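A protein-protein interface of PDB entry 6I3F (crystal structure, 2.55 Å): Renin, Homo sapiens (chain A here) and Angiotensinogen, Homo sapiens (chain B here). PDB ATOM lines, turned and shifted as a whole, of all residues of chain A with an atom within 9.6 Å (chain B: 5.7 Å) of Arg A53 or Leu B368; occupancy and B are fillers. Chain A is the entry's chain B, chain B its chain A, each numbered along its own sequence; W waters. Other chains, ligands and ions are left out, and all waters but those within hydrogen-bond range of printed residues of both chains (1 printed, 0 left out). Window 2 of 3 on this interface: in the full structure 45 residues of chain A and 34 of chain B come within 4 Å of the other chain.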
ATOM      1  N   SER A  48       3.656  30.654  -2.080  1.00  0.00           N
ATOM      2  CA  SER A  48       4.722  31.321  -2.875  1.00  0.00           C
ATOM      3  C   SER A  48       4.137  31.914  -4.163  1.00  0.00           C
ATOM      4  O   SER A  48       3.192  31.317  -4.715  1.00  0.00           O
ATOM      5  CB  SER A  48       5.825  30.345  -3.192  1.00  0.00           C
ATOM      6  OG  SER A  48       6.899  30.985  -3.869  1.00  0.00           O
ATOM      7  N   SER A  49       4.706  33.027  -4.638  1.00  0.00           N
ATOM      8  CA  SER A  49       4.446  33.608  -5.983  1.00  0.00           C
ATOM      9  C   SER A  49       4.837  32.598  -7.072  1.00  0.00           C
ATOM     10  O   SER A  49       4.242  32.652  -8.163  1.00  0.00           O
ATOM     11  CB  SER A  49       5.181  34.913  -6.167  1.00  0.00           C
ATOM     12  OG  SER A  49       6.584  34.701  -6.217  1.00  0.00           O
ATOM     13  N   LYS A  50       5.793  31.709  -6.770  1.00  0.00           N
ATOM     14  CA  LYS A  50       6.310  30.659  -7.693  1.00  0.00           C
ATOM     15  C   LYS A  50       5.366  29.449  -7.725  1.00  0.00           C
ATOM     16  O   LYS A  50       5.662  28.506  -8.488  1.00  0.00           O
ATOM     17  CB  LYS A  50       7.711  30.204  -7.272  1.00  0.00           C
ATOM     18  CG  LYS A  50       8.730  31.317  -7.071  1.00  0.00           C
ATOM     19  CD  LYS A  50      10.155  30.908  -7.407  1.00  0.00           C
ATOM     20  CE  LYS A  50      11.211  31.661  -6.620  1.00  0.00           C
ATOM     21  NZ  LYS A  50      10.931  33.117  -6.540  1.00  0.00           N
ATOM     22  N   CYS A  51       4.293  29.449  -6.926  1.00  0.00           N
ATOM     23  CA  CYS A  51       3.235  28.404  -6.954  1.00  0.00           C
ATOM     24  C   CYS A  51       2.449  28.521  -8.263  1.00  0.00           C
ATOM     25  O   CYS A  51       1.909  29.612  -8.526  1.00  0.00           O
ATOM     26  CB  CYS A  51       2.270  28.516  -5.780  1.00  0.00           C
ATOM     27  SG  CYS A  51       1.057  27.170  -5.754  1.00  0.00           S
ATOM     28  N   SER A  52       2.394  27.434  -9.040  1.00  0.00           N
ATOM     29  CA  SER A  52       1.683  27.348 -10.343  1.00  0.00           C
ATOM     30  C   SER A  52       0.223  27.778 -10.163  1.00  0.00           C
ATOM     31  O   SER A  52      -0.366  27.465  -9.107  1.00  0.00           O
ATOM     32  CB  SER A  52       1.779  25.958 -10.927  1.00  0.00           C
ATOM     33  OG  SER A  52       0.989  25.846 -12.104  1.00  0.00           O
ATOM     34  N   ARG A  53      -0.328  28.466 -11.166  1.00  0.00           N
ATOM     35  CA  ARG A  53      -1.734  28.950 -11.182  1.00  0.00           C
ATOM     36  C   ARG A  53      -2.693  27.756 -11.286  1.00  0.00           C
ATOM     37  O   ARG A  53      -3.887  27.951 -11.015  1.00  0.00           O
ATOM     38  CB  ARG A  53      -1.946  29.945 -12.329  1.00  0.00           C
ATOM     39  CG  ARG A  53      -1.263  31.289 -12.112  1.00  0.00           C
ATOM     40  CD  ARG A  53      -1.229  32.139 -13.370  1.00  0.00           C
ATOM     41  NE  ARG A  53      -0.455  31.505 -14.432  1.00  0.00           N
ATOM     42  CZ  ARG A  53      -0.449  31.882 -15.712  1.00  0.00           C
ATOM     43  NH1 ARG A  53       0.294  31.220 -16.585  1.00  0.00           N
ATOM     44  NH2 ARG A  53      -1.182  32.908 -16.117  1.00  0.00           N
ATOM     45  N   LEU A  54      -2.196  26.571 -11.653  1.00  0.00           N
ATOM     46  CA  LEU A  54      -2.996  25.316 -11.703  1.00  0.00           C
ATOM     47  C   LEU A  54      -3.589  25.022 -10.318  1.00  0.00           C
ATOM     48  O   LEU A  54      -4.753  24.588 -10.261  1.00  0.00           O
ATOM     49  CB  LEU A  54      -2.108  24.164 -12.187  1.00  0.00           C
ATOM     50  CG  LEU A  54      -1.693  24.224 -13.657  1.00  0.00           C
ATOM     51  CD1 LEU A  54      -0.668  23.150 -13.971  1.00  0.00           C
ATOM     52  CD2 LEU A  54      -2.895  24.087 -14.582  1.00  0.00           C
ATOM     53  N   TYR A  55      -2.828  25.270  -9.248  1.00  0.00           N
ATOM     54  CA  TYR A  55      -3.252  25.055  -7.838  1.00  0.00           C
ATOM     55  C   TYR A  55      -4.246  26.152  -7.436  1.00  0.00           C
ATOM     56  O   TYR A  55      -3.818  27.279  -7.109  1.00  0.00           O
ATOM     57  CB  TYR A  55      -2.037  24.994  -6.908  1.00  0.00           C
ATOM     58  CG  TYR A  55      -1.128  23.826  -7.185  1.00  0.00           C
ATOM     59  CD1 TYR A  55       0.100  24.001  -7.803  1.00  0.00           C
ATOM     60  CD2 TYR A  55      -1.518  22.534  -6.870  1.00  0.00           C
ATOM     61  CE1 TYR A  55       0.928  22.925  -8.078  1.00  0.00           C
ATOM     62  CE2 TYR A  55      -0.704  21.446  -7.141  1.00  0.00           C
ATOM     63  CZ  TYR A  55       0.523  21.643  -7.748  1.00  0.00           C
ATOM     64  OH  TYR A  55       1.329  20.576  -8.013  1.00  0.00           O
ATOM     65  N   THR A  56      -5.540  25.816  -7.470  1.00  0.00           N
ATOM     66  CA  THR A  56      -6.677  26.685  -7.065  1.00  0.00           C
ATOM     67  C   THR A  56      -6.393  27.295  -5.685  1.00  0.00           C
ATOM     68  O   THR A  56      -6.641  28.502  -5.515  1.00  0.00           O
ATOM     69  CB  THR A  56      -7.985  25.882  -7.086  1.00  0.00           C
ATOM     70  OG1 THR A  56      -8.096  25.281  -8.375  1.00  0.00           O
ATOM     71  CG2 THR A  56      -9.213  26.720  -6.801  1.00  0.00           C
ATOM     72  N   ALA A  57      -5.873  26.491  -4.750  1.00  0.00           N
ATOM     73  CA  ALA A  57      -5.616  26.859  -3.336  1.00  0.00           C
ATOM     74  C   ALA A  57      -4.603  28.009  -3.242  1.00  0.00           C
ATOM     75  O   ALA A  57      -4.736  28.820  -2.312  1.00  0.00           O
ATOM     76  CB  ALA A  57      -5.152  25.647  -2.565  1.00  0.00           C
ATOM     77  N   CYS A  58      -3.629  28.079  -4.158  1.00  0.00           N
ATOM     78  CA  CYS A  58      -2.633  29.184  -4.251  1.00  0.00           C
ATOM     79  C   CYS A  58      -3.313  30.454  -4.773  1.00  0.00           C
ATOM     80  O   CYS A  58      -3.078  31.532  -4.193  1.00  0.00           O
ATOM     81  CB  CYS A  58      -1.453  28.814  -5.143  1.00  0.00           C
ATOM     82  SG  CYS A  58      -0.282  27.698  -4.329  1.00  0.00           S
ATOM     83  N   VAL A  59      -4.144  30.323  -5.809  1.00  0.00           N
ATOM     84  CA  VAL A  59      -4.795  31.464  -6.521  1.00  0.00           C
ATOM     85  C   VAL A  59      -5.722  32.222  -5.555  1.00  0.00           C
ATOM     86  O   VAL A  59      -5.849  33.448  -5.724  1.00  0.00           O
ATOM     87  CB  VAL A  59      -5.545  30.979  -7.777  1.00  0.00           C
ATOM     88  CG1 VAL A  59      -6.302  32.108  -8.463  1.00  0.00           C
ATOM     89  CG2 VAL A  59      -4.606  30.298  -8.762  1.00  0.00           C
ATOM     90  N   TYR A  60      -6.335  31.536  -4.582  1.00  0.00           N
ATOM     91  CA  TYR A  60      -7.358  32.108  -3.662  1.00  0.00           C
ATOM     92  C   TYR A  60      -6.758  32.385  -2.277  1.00  0.00           C
ATOM     93  O   TYR A  60      -7.532  32.499  -1.303  1.00  0.00           O
ATOM     94  CB  TYR A  60      -8.582  31.190  -3.598  1.00  0.00           C
ATOM     95  CG  TYR A  60      -9.430  31.243  -4.843  1.00  0.00           C
ATOM     96  CD1 TYR A  60      -9.288  30.300  -5.848  1.00  0.00           C
ATOM     97  CD2 TYR A  60     -10.345  32.264  -5.039  1.00  0.00           C
ATOM     98  CE1 TYR A  60     -10.048  30.354  -7.005  1.00  0.00           C
ATOM     99  CE2 TYR A  60     -11.114  32.335  -6.189  1.00  0.00           C
ATOM    100  CZ  TYR A  60     -10.965  31.376  -7.176  1.00  0.00           C
ATOM    101  OH  TYR A  60     -11.717  31.435  -8.314  1.00  0.00           O
ATOM    102  N   LEU A  63       0.117  35.349  -1.868  1.00  0.00           N
ATOM    103  CA  LEU A  63       1.399  34.725  -2.291  1.00  0.00           C
ATOM    104  C   LEU A  63       2.566  35.619  -1.854  1.00  0.00           C
ATOM    105  O   LEU A  63       2.420  36.854  -1.920  1.00  0.00           O
ATOM    106  CB  LEU A  63       1.379  34.534  -3.812  1.00  0.00           C
ATOM    107  CG  LEU A  63       0.176  33.768  -4.362  1.00  0.00           C
ATOM    108  CD1 LEU A  63       0.269  33.623  -5.873  1.00  0.00           C
ATOM    109  CD2 LEU A  63       0.051  32.403  -3.701  1.00  0.00           C
ATOM    110  N   THR A 112       4.843  25.862  -3.034  1.00  0.00           N
ATOM    111  CA  THR A 112       4.626  25.890  -4.507  1.00  0.00           C
ATOM    112  C   THR A 112       3.613  24.815  -4.928  1.00  0.00           C
ATOM    113  O   THR A 112       3.232  24.820  -6.114  1.00  0.00           O
ATOM    114  CB  THR A 112       5.956  25.725  -5.251  1.00  0.00           C
ATOM    115  OG1 THR A 112       6.547  24.486  -4.859  1.00  0.00           O
ATOM    116  CG2 THR A 112       6.923  26.855  -4.977  1.00  0.00           C
ATOM    117  N   GLU A 113       3.194  23.932  -4.013  1.00  0.00           N
ATOM    118  CA  GLU A 113       2.184  22.870  -4.272  1.00  0.00           C
ATOM    119  C   GLU A 113       1.216  22.793  -3.082  1.00  0.00           C
ATOM    120  O   GLU A 113       1.670  22.483  -1.963  1.00  0.00           O
ATOM    121  CB  GLU A 113       2.873  21.530  -4.538  1.00  0.00           C
ATOM    122  CG  GLU A 113       3.971  21.616  -5.587  1.00  0.00           C
ATOM    123  CD  GLU A 113       4.395  20.292  -6.207  1.00  0.00           C
ATOM    124  OE1 GLU A 113       4.202  19.241  -5.558  1.00  0.00           O
ATOM    125  OE2 GLU A 113       4.918  20.317  -7.345  1.00  0.00           O
ATOM    126  N   MET A 114      -0.066  23.082  -3.327  1.00  0.00           N
ATOM    127  CA  MET A 114      -1.154  23.082  -2.313  1.00  0.00           C
ATOM    128  C   MET A 114      -2.348  22.300  -2.855  1.00  0.00           C
ATOM    129  O   MET A 114      -2.895  22.650  -3.898  1.00  0.00           O
ATOM    130  CB  MET A 114      -1.597  24.510  -1.976  1.00  0.00           C
ATOM    131  CG  MET A 114      -1.039  25.027  -0.664  1.00  0.00           C
ATOM    132  SD  MET A 114      -1.873  26.523  -0.069  1.00  0.00           S
ATOM    133  CE  MET A 114      -1.328  27.698  -1.303  1.00  0.00           C
ATOM    134  N   ARG B  83     -14.243  28.309  -9.811  1.00  0.00           N
ATOM    135  CA  ARG B  83     -13.074  28.925 -10.485  1.00  0.00           C
ATOM    136  C   ARG B  83     -13.385  29.108 -11.974  1.00  0.00           C
ATOM    137  O   ARG B  83     -13.250  30.241 -12.469  1.00  0.00           O
ATOM    138  CB  ARG B  83     -11.814  28.080 -10.284  1.00  0.00           C
ATOM    139  CG  ARG B  83     -10.540  28.838 -10.620  1.00  0.00           C
ATOM    140  CD  ARG B  83      -9.295  27.985 -10.568  1.00  0.00           C
ATOM    141  NE  ARG B  83      -8.167  28.743 -11.081  1.00  0.00           N
ATOM    142  CZ  ARG B  83      -6.935  28.273 -11.214  1.00  0.00           C
ATOM    143  NH1 ARG B  83      -6.645  27.028 -10.869  1.00  0.00           N
ATOM    144  NH2 ARG B  83      -5.990  29.058 -11.701  1.00  0.00           N
ATOM    145  N   MET B  87     -13.969  32.306 -14.577  1.00  0.00           N
ATOM    146  CA  MET B  87     -13.234  32.485 -15.858  1.00  0.00           C
ATOM    147  C   MET B  87     -14.230  32.828 -16.968  1.00  0.00           C
ATOM    148  O   MET B  87     -13.980  33.808 -17.695  1.00  0.00           O
ATOM    149  CB  MET B  87     -12.472  31.217 -16.252  1.00  0.00           C
ATOM    150  CG  MET B  87     -11.295  30.932 -15.355  1.00  0.00           C
ATOM    151  SD  MET B  87     -10.508  29.356 -15.738  1.00  0.00           S
ATOM    152  CE  MET B  87      -9.232  29.330 -14.480  1.00  0.00           C
ATOM    153  N   ILE B 128      -4.748  20.780 -11.279  1.00  0.00           N
ATOM    154  CA  ILE B 128      -5.944  21.663 -11.454  1.00  0.00           C
ATOM    155  C   ILE B 128      -7.189  20.978 -10.875  1.00  0.00           C
ATOM    156  O   ILE B 128      -8.074  21.705 -10.386  1.00  0.00           O
ATOM    157  CB  ILE B 128      -6.149  22.099 -12.922  1.00  0.00           C
ATOM    158  CG1 ILE B 128      -7.066  23.320 -13.007  1.00  0.00           C
ATOM    159  CG2 ILE B 128      -6.658  20.957 -13.789  1.00  0.00           C
ATOM    160  CD1 ILE B 128      -6.994  24.050 -14.325  1.00  0.00           C
ATOM    161  N   LEU B 363     -10.031  27.614 -21.060  1.00  0.00           N
ATOM    162  CA  LEU B 363      -8.757  27.352 -20.332  1.00  0.00           C
ATOM    163  C   LEU B 363      -7.588  28.036 -21.051  1.00  0.00           C
ATOM    164  O   LEU B 363      -6.701  28.563 -20.353  1.00  0.00           O
ATOM    165  CB  LEU B 363      -8.522  25.839 -20.233  1.00  0.00           C
ATOM    166  CG  LEU B 363      -9.480  25.074 -19.321  1.00  0.00           C
ATOM    167  CD1 LEU B 363      -9.258  23.575 -19.443  1.00  0.00           C
ATOM    168  CD2 LEU B 363      -9.332  25.514 -17.874  1.00  0.00           C
ATOM    169  N   ALA B 366      -7.755  31.821 -20.343  1.00  0.00           N
ATOM    170  CA  ALA B 366      -7.701  32.126 -18.893  1.00  0.00           C
ATOM    171  C   ALA B 366      -6.239  32.268 -18.450  1.00  0.00           C
ATOM    172  O   ALA B 366      -5.336  31.963 -19.256  1.00  0.00           O
ATOM    173  CB  ALA B 366      -8.415  31.051 -18.111  1.00  0.00           C
ATOM    174  N   GLU B 367      -6.030  32.717 -17.208  1.00  0.00           N
ATOM    175  CA  GLU B 367      -4.690  32.904 -16.585  1.00  0.00           C
ATOM    176  C   GLU B 367      -4.189  31.544 -16.083  1.00  0.00           C
ATOM    177  O   GLU B 367      -4.209  31.319 -14.855  1.00  0.00           O
ATOM    178  CB  GLU B 367      -4.765  33.942 -15.461  1.00  0.00           C
ATOM    179  CG  GLU B 367      -5.267  35.303 -15.915  1.00  0.00           C
ATOM    180  CD  GLU B 367      -4.481  35.930 -17.055  1.00  0.00           C
ATOM    181  OE1 GLU B 367      -3.233  35.906 -16.995  1.00  0.00           O
ATOM    182  OE2 GLU B 367      -5.116  36.426 -18.012  1.00  0.00           O
ATOM    183  N   LEU B 368      -3.773  30.675 -17.012  1.00  0.00           N
ATOM    184  CA  LEU B 368      -3.287  29.296 -16.734  1.00  0.00           C
ATOM    185  C   LEU B 368      -2.111  28.969 -17.651  1.00  0.00           C
ATOM    186  O   LEU B 368      -1.976  29.555 -18.723  1.00  0.00           O
ATOM    187  CB  LEU B 368      -4.428  28.300 -16.971  1.00  0.00           C
ATOM    188  CG  LEU B 368      -5.544  28.292 -15.929  1.00  0.00           C
ATOM    189  CD1 LEU B 368      -6.674  27.373 -16.367  1.00  0.00           C
ATOM    190  CD2 LEU B 368      -5.018  27.873 -14.564  1.00  0.00           C
ATOM    191  N   PRO B 369      -1.228  28.018 -17.260  1.00  0.00           N
ATOM    192  CA  PRO B 369      -0.312  27.389 -18.209  1.00  0.00           C
ATOM    193  C   PRO B 369      -1.081  26.441 -19.143  1.00  0.00           C
ATOM    194  O   PRO B 369      -2.196  26.070 -18.816  1.00  0.00           O
ATOM    195  CB  PRO B 369       0.681  26.634 -17.313  1.00  0.00           C
ATOM    196  CG  PRO B 369      -0.107  26.340 -16.053  1.00  0.00           C
ATOM    197  CD  PRO B 369      -1.051  27.513 -15.890  1.00  0.00           C
ATOM    198  N   ALA B 370      -0.472  26.084 -20.278  1.00  0.00           N
ATOM    199  CA  ALA B 370      -1.070  25.233 -21.333  1.00  0.00           C
ATOM    200  C   ALA B 370      -1.250  23.802 -20.810  1.00  0.00           C
ATOM    201  O   ALA B 370      -0.296  23.265 -20.212  1.00  0.00           O
ATOM    202  CB  ALA B 370      -0.205  25.267 -22.570  1.00  0.00           C
ATOM    203  N   ILE B 371      -2.437  23.221 -21.028  1.00  0.00           N
ATOM    204  CA  ILE B 371      -2.786  21.813 -20.668  1.00  0.00           C
ATOM    205  C   ILE B 371      -3.084  21.029 -21.953  1.00  0.00           C
ATOM    206  O   ILE B 371      -2.445  19.977 -22.158  1.00  0.00           O
ATOM    207  CB  ILE B 371      -3.972  21.767 -19.683  1.00  0.00           C
ATOM    208  CG1 ILE B 371      -3.686  22.568 -18.408  1.00  0.00           C
ATOM    209  CG2 ILE B 371      -4.354  20.327 -19.366  1.00  0.00           C
ATOM    210  CD1 ILE B 371      -4.920  22.908 -17.604  1.00  0.00           C
HETATM  211  O   HOH W   1      -8.888  22.970  -8.178  1.00  0.00           O
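The guanidinium group of Arg B83 lies within hydrogen-bond range of the backbone carbonyl oxygen of Arg A53 (2.5 Å).
The guanidinium group (NH1) of Arg B83 is in hydrogen-bond range of the backbone carbonyl oxygen (O) of Leu A54, at 3.1 Å.
The guanidinium group of Arg B83 lies within hydrogen-bond range of the side-chain hydroxyl of Thr A56, at 3.4 Å.
The guanidinium group (NH2) of Arg A53 is in salt-bridge range of the side-chain carboxylate (OE1) of Glu B367, 3.7 Å away.
The backbone NH of Leu A54 sits close to the side-chain hydroxyl of Ser A52 (3.3 Å).
SG of Cys A51 is disulfide-bonded to SG of Cys A58, 2.0 Å away.
Among the printed residues, pairs that only touch across the chains: Arg A53 with Leu B368 (3.5 Å), Arg A53 with Pro B369 (3.6 Å), Leu A54 with Ile B128 (3.4 Å), Leu A54 with Pro B369 (3.6 Å), Leu A54 with Ile B371 (3.8 Å), Val A59 with Arg B83 (3.5 Å) and Tyr A60 with Arg B83 (3.6 Å).
Ser A49 touches none of the printed residues of chain B.
Of chain B, only Arg B83, Glu B367, Leu B368 and Pro B369 come within 4 Å of Arg A53.
Of the printed residues of chain B, Thr A56 touches Arg B83.
Ala A57 touches none of the printed residues of chain B.
Of the printed residues of chain B, Tyr A60 touches Arg B83 (3.6 Å).
Of the printed residues of chain A, Arg B83 touches Arg A53 (2.5 Å), Leu A54 (3.1 Å), Thr A56 (3.4 Å), Val A59 (3.5 Å) and Tyr A60 (3.6 Å).
Printed residues of chain A within 4 Å of Ile B128: Leu A54 (3.4 Å).
Printed residues of chain A within 4 Å of Glu B367: Arg A53 (3.3 Å).
Of the printed residues of chain A, Leu B368 touches Arg A53.
The nearest residue of chain B that does not touch Arg A53 is Ala B366 (5.3 Å).
The nearest residue of chain A that does not touch Leu B368 is Leu A54 (4.3 Å).
The nearest printed residue of chain A that does not touch Glu B367 is Leu A54 (6.1 Å).
Of the 17 printed residues of chain A, 5 touch a printed residue of chain B.
Hydrophobic or aromatic side chains of chain A that line the printed part of chain B: Leu A54, Val A59 and Tyr A60.
Among the printed residues, 11 pairs touch across the chains.
Among the printed residues, Asp or Glu carboxylates within 4 Å of a Lys or Arg side-chain nitrogen of the other chain: Arg A53 with Glu B367 (3.7 Å).
Water W1 bridges OG1 of Thr A56 (2.5 Å) and O of Ile B128 (2.7 Å).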
